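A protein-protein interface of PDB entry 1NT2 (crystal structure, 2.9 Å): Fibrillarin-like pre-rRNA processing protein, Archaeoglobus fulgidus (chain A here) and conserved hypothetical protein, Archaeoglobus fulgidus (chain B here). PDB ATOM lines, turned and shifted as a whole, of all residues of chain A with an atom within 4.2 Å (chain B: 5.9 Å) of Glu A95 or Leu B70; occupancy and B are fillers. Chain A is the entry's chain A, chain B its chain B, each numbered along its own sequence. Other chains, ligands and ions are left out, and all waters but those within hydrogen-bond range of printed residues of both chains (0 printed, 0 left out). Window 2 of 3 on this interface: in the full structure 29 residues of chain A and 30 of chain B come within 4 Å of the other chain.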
ATOM      1  N   ALA A  91      24.596   9.049  -7.702  1.00  0.00           N
ATOM      2  CA  ALA A  91      23.913   9.802  -6.663  1.00  0.00           C
ATOM      3  C   ALA A  91      22.625  10.465  -7.139  1.00  0.00           C
ATOM      4  O   ALA A  91      21.622  10.438  -6.431  1.00  0.00           O
ATOM      5  CB  ALA A  91      24.853  10.843  -6.075  1.00  0.00           C
ATOM      6  N   LYS A  92      22.641  11.055  -8.329  1.00  0.00           N
ATOM      7  CA  LYS A  92      21.453  11.727  -8.848  1.00  0.00           C
ATOM      8  C   LYS A  92      20.165  10.931  -8.590  1.00  0.00           C
ATOM      9  O   LYS A  92      19.289  11.369  -7.836  1.00  0.00           O
ATOM     10  CB  LYS A  92      21.614  11.997 -10.350  1.00  0.00           C
ATOM     11  CG  LYS A  92      20.364  12.544 -11.058  1.00  0.00           C
ATOM     12  CD  LYS A  92      20.076  14.007 -10.714  1.00  0.00           C
ATOM     13  CE  LYS A  92      18.829  14.525 -11.443  1.00  0.00           C
ATOM     14  NZ  LYS A  92      17.573  13.824 -11.018  1.00  0.00           N
ATOM     15  N   PRO A  93      20.047   9.738  -9.189  1.00  0.00           N
ATOM     16  CA  PRO A  93      18.857   8.905  -9.013  1.00  0.00           C
ATOM     17  C   PRO A  93      18.736   8.395  -7.589  1.00  0.00           C
ATOM     18  O   PRO A  93      17.642   8.276  -7.035  1.00  0.00           O
ATOM     19  CB  PRO A  93      19.107   7.773  -9.986  1.00  0.00           C
ATOM     20  CG  PRO A  93      20.577   7.566  -9.841  1.00  0.00           C
ATOM     21  CD  PRO A  93      21.108   8.979  -9.874  1.00  0.00           C
ATOM     22  N   PHE A  94      19.888   8.087  -7.012  1.00  0.00           N
ATOM     23  CA  PHE A  94      19.958   7.560  -5.667  1.00  0.00           C
ATOM     24  C   PHE A  94      19.309   8.512  -4.686  1.00  0.00           C
ATOM     25  O   PHE A  94      18.691   8.083  -3.723  1.00  0.00           O
ATOM     26  CB  PHE A  94      21.416   7.325  -5.272  1.00  0.00           C
ATOM     27  CG  PHE A  94      21.586   6.300  -4.201  1.00  0.00           C
ATOM     28  CD1 PHE A  94      21.573   4.945  -4.514  1.00  0.00           C
ATOM     29  CD2 PHE A  94      21.678   6.683  -2.866  1.00  0.00           C
ATOM     30  CE1 PHE A  94      21.643   3.983  -3.512  1.00  0.00           C
ATOM     31  CE2 PHE A  94      21.747   5.732  -1.857  1.00  0.00           C
ATOM     32  CZ  PHE A  94      21.728   4.377  -2.179  1.00  0.00           C
ATOM     33  N   GLU A  95      19.447   9.808  -4.924  1.00  0.00           N
ATOM     34  CA  GLU A  95      18.865  10.781  -4.025  1.00  0.00           C
ATOM     35  C   GLU A  95      17.377  10.514  -3.901  1.00  0.00           C
ATOM     36  O   GLU A  95      16.809  10.623  -2.821  1.00  0.00           O
ATOM     37  CB  GLU A  95      19.119  12.193  -4.547  1.00  0.00           C
ATOM     38  CG  GLU A  95      18.542  13.292  -3.666  1.00  0.00           C
ATOM     39  CD  GLU A  95      18.816  14.695  -4.207  1.00  0.00           C
ATOM     40  OE1 GLU A  95      18.657  14.912  -5.432  1.00  0.00           O
ATOM     41  OE2 GLU A  95      19.179  15.585  -3.401  1.00  0.00           O
ATOM     42  N   LYS A  96      16.754  10.146  -5.016  1.00  0.00           N
ATOM     43  CA  LYS A  96      15.324   9.853  -5.053  1.00  0.00           C
ATOM     44  C   LYS A  96      15.030   8.485  -4.457  1.00  0.00           C
ATOM     45  O   LYS A  96      13.931   8.245  -3.964  1.00  0.00           O
ATOM     46  CB  LYS A  96      14.812   9.890  -6.500  1.00  0.00           C
ATOM     47  CG  LYS A  96      13.317   9.578  -6.677  1.00  0.00           C
ATOM     48  CD  LYS A  96      12.451  10.587  -5.931  1.00  0.00           C
ATOM     49  CE  LYS A  96      11.015  10.663  -6.456  1.00  0.00           C
ATOM     50  NZ  LYS A  96      10.313  11.881  -5.907  1.00  0.00           N
ATOM     51  N   LEU A  97      16.015   7.592  -4.511  1.00  0.00           N
ATOM     52  CA  LEU A  97      15.861   6.235  -3.986  1.00  0.00           C
ATOM     53  C   LEU A  97      15.650   6.229  -2.477  1.00  0.00           C
ATOM     54  O   LEU A  97      14.722   5.590  -1.977  1.00  0.00           O
ATOM     55  CB  LEU A  97      17.093   5.375  -4.323  1.00  0.00           C
ATOM     56  CG  LEU A  97      16.988   3.860  -4.078  1.00  0.00           C
ATOM     57  CD1 LEU A  97      16.212   3.183  -5.200  1.00  0.00           C
ATOM     58  CD2 LEU A  97      18.367   3.256  -3.994  1.00  0.00           C
ATOM     59  N   LEU A  98      16.510   6.939  -1.757  1.00  0.00           N
ATOM     60  CA  LEU A  98      16.427   7.003  -0.298  1.00  0.00           C
ATOM     61  C   LEU A  98      15.027   7.325   0.206  1.00  0.00           C
ATOM     62  O   LEU A  98      14.645   6.913   1.300  1.00  0.00           O
ATOM     63  CB  LEU A  98      17.425   8.035   0.259  1.00  0.00           C
ATOM     64  CG  LEU A  98      18.916   7.669   0.306  1.00  0.00           C
ATOM     65  CD1 LEU A  98      19.686   8.808   0.940  1.00  0.00           C
ATOM     66  CD2 LEU A  98      19.124   6.400   1.108  1.00  0.00           C
ATOM     67  N   MET B  65      26.487  10.234   1.294  1.00  0.00           N
ATOM     68  CA  MET B  65      26.878  10.365  -0.100  1.00  0.00           C
ATOM     69  C   MET B  65      26.055  11.481  -0.719  1.00  0.00           C
ATOM     70  O   MET B  65      26.594  12.442  -1.267  1.00  0.00           O
ATOM     71  CB  MET B  65      26.619   9.072  -0.867  1.00  0.00           C
ATOM     72  CG  MET B  65      26.876   9.212  -2.351  1.00  0.00           C
ATOM     73  SD  MET B  65      25.666   8.314  -3.319  1.00  0.00           S
ATOM     74  CE  MET B  65      26.659   6.924  -3.892  1.00  0.00           C
ATOM     75  N   VAL B  66      24.739  11.352  -0.617  1.00  0.00           N
ATOM     76  CA  VAL B  66      23.848  12.348  -1.176  1.00  0.00           C
ATOM     77  C   VAL B  66      24.114  13.692  -0.518  1.00  0.00           C
ATOM     78  O   VAL B  66      23.895  14.738  -1.119  1.00  0.00           O
ATOM     79  CB  VAL B  66      22.387  11.928  -0.985  1.00  0.00           C
ATOM     80  CG1 VAL B  66      21.474  12.814  -1.808  1.00  0.00           C
ATOM     81  CG2 VAL B  66      22.223  10.485  -1.407  1.00  0.00           C
ATOM     82  N   GLU B  67      24.611  13.669   0.712  1.00  0.00           N
ATOM     83  CA  GLU B  67      24.910  14.915   1.405  1.00  0.00           C
ATOM     84  C   GLU B  67      26.118  15.615   0.773  1.00  0.00           C
ATOM     85  O   GLU B  67      26.091  16.824   0.533  1.00  0.00           O
ATOM     86  CB  GLU B  67      25.178  14.658   2.888  1.00  0.00           C
ATOM     87  CG  GLU B  67      25.029  15.901   3.734  1.00  0.00           C
ATOM     88  CD  GLU B  67      23.671  16.566   3.535  1.00  0.00           C
ATOM     89  OE1 GLU B  67      23.415  17.597   4.192  1.00  0.00           O
ATOM     90  OE2 GLU B  67      22.860  16.062   2.721  1.00  0.00           O
ATOM     91  N   LYS B  68      27.175  14.852   0.505  1.00  0.00           N
ATOM     92  CA  LYS B  68      28.368  15.406  -0.122  1.00  0.00           C
ATOM     93  C   LYS B  68      28.049  15.842  -1.555  1.00  0.00           C
ATOM     94  O   LYS B  68      28.339  16.974  -1.937  1.00  0.00           O
ATOM     95  CB  LYS B  68      29.497  14.374  -0.145  1.00  0.00           C
ATOM     96  CG  LYS B  68      30.117  14.067   1.199  1.00  0.00           C
ATOM     97  CD  LYS B  68      31.204  13.015   1.043  1.00  0.00           C
ATOM     98  CE  LYS B  68      31.794  12.592   2.382  1.00  0.00           C
ATOM     99  NZ  LYS B  68      32.542  13.694   3.034  1.00  0.00           N
ATOM    100  N   GLU B  69      27.449  14.945  -2.339  1.00  0.00           N
ATOM    101  CA  GLU B  69      27.106  15.243  -3.730  1.00  0.00           C
ATOM    102  C   GLU B  69      26.173  16.429  -3.860  1.00  0.00           C
ATOM    103  O   GLU B  69      25.842  16.847  -4.967  1.00  0.00           O
ATOM    104  CB  GLU B  69      26.472  14.031  -4.418  1.00  0.00           C
ATOM    105  CG  GLU B  69      27.428  12.873  -4.603  1.00  0.00           C
ATOM    106  CD  GLU B  69      28.755  13.306  -5.202  1.00  0.00           C
ATOM    107  OE1 GLU B  69      28.766  13.835  -6.338  1.00  0.00           O
ATOM    108  OE2 GLU B  69      29.790  13.118  -4.529  1.00  0.00           O
ATOM    109  N   LEU B  70      25.733  16.957  -2.727  1.00  0.00           N
ATOM    110  CA  LEU B  70      24.861  18.121  -2.733  1.00  0.00           C
ATOM    111  C   LEU B  70      25.792  19.326  -2.588  1.00  0.00           C
ATOM    112  O   LEU B  70      25.558  20.390  -3.161  1.00  0.00           O
ATOM    113  CB  LEU B  70      23.899  18.067  -1.550  1.00  0.00           C
ATOM    114  CG  LEU B  70      22.722  19.030  -1.669  1.00  0.00           C
ATOM    115  CD1 LEU B  70      21.650  18.380  -2.546  1.00  0.00           C
ATOM    116  CD2 LEU B  70      22.173  19.367  -0.284  1.00  0.00           C
ATOM    117  N   ARG B  71      26.856  19.126  -1.813  1.00  0.00           N
ATOM    118  CA  ARG B  71      27.868  20.143  -1.560  1.00  0.00           C
ATOM    119  C   ARG B  71      28.862  20.223  -2.718  1.00  0.00           C
ATOM    120  O   ARG B  71      29.475  21.262  -2.945  1.00  0.00           O
ATOM    121  CB  ARG B  71      28.633  19.812  -0.272  1.00  0.00           C
ATOM    122  CG  ARG B  71      27.967  20.261   1.022  1.00  0.00           C
ATOM    123  CD  ARG B  71      28.796  19.839   2.242  1.00  0.00           C
ATOM    124  NE  ARG B  71      28.593  18.434   2.606  1.00  0.00           N
ATOM    125  CZ  ARG B  71      29.236  17.804   3.591  1.00  0.00           C
ATOM    126  NH1 ARG B  71      30.138  18.448   4.318  1.00  0.00           N
ATOM    127  NH2 ARG B  71      28.970  16.531   3.864  1.00  0.00           N
ATOM    128  N   ARG B  72      29.016  19.112  -3.438  1.00  0.00           N
ATOM    129  CA  ARG B  72      29.938  18.997  -4.575  1.00  0.00           C
ATOM    130  C   ARG B  72      31.347  19.519  -4.281  1.00  0.00           C
ATOM    131  O   ARG B  72      32.095  19.879  -5.189  1.00  0.00           O
ATOM    132  CB  ARG B  72      29.365  19.698  -5.814  1.00  0.00           C
ATOM    133  CG  ARG B  72      28.211  18.941  -6.479  1.00  0.00           C
ATOM    134  CD  ARG B  72      27.938  19.423  -7.919  1.00  0.00           C
ATOM    135  NE  ARG B  72      27.587  20.848  -8.016  1.00  0.00           N
ATOM    136  CZ  ARG B  72      27.311  21.478  -9.159  1.00  0.00           C
ATOM    137  NH1 ARG B  72      27.345  20.810 -10.306  1.00  0.00           N
ATOM    138  NH2 ARG B  72      27.005  22.774  -9.158  1.00  0.00           N
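Among the printed residues, pairs that only touch across the chains: Ala A91 with Met B65 (3.8 Å), Ala A91 with Glu B69 (3.6 Å), Glu A95 with Val B66 (3.5 Å), Glu A95 with Leu B70 (3.8 Å) and Leu A98 with Val B66 (3.8 Å).
Printed residues of chain A that touch a printed residue of chain B: Ala A91, Glu A95 and Leu A98.
Hydrophobic or aromatic side chains of chain A within 4 Å of the printed part of chain B: Ala A91 and Leu A98.
Of the 8 printed residues of chain B, 4 touch a printed residue of chain A.
Among the printed residues, no Asp or Glu carboxylate lies within 4 Å of a Lys or Arg side-chain nitrogen of the other chain.
Of the printed residues of chain B, Ala A91 touches Met B65 (3.8 Å) and Glu B69 (3.6 Å).
Of chain B, only Val B66 (3.5 Å) and Leu B70 (3.8 Å) come within 4 Å of Glu A95.
Lys A96 touches none of the printed residues of chain B.
Of the printed residues of chain A, Val B66 touches Glu A95 (3.5 Å) and Leu A98 (3.8 Å).
Leu B70 touches just one residue of chain A: Glu A95 (3.8 Å).
The nearest printed residue of chain B that does not touch Glu A95 is Met B65 (6.6 Å).
The nearest printed residue of chain A that does not touch Leu B70 is Ala A91 (7.0 Å).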
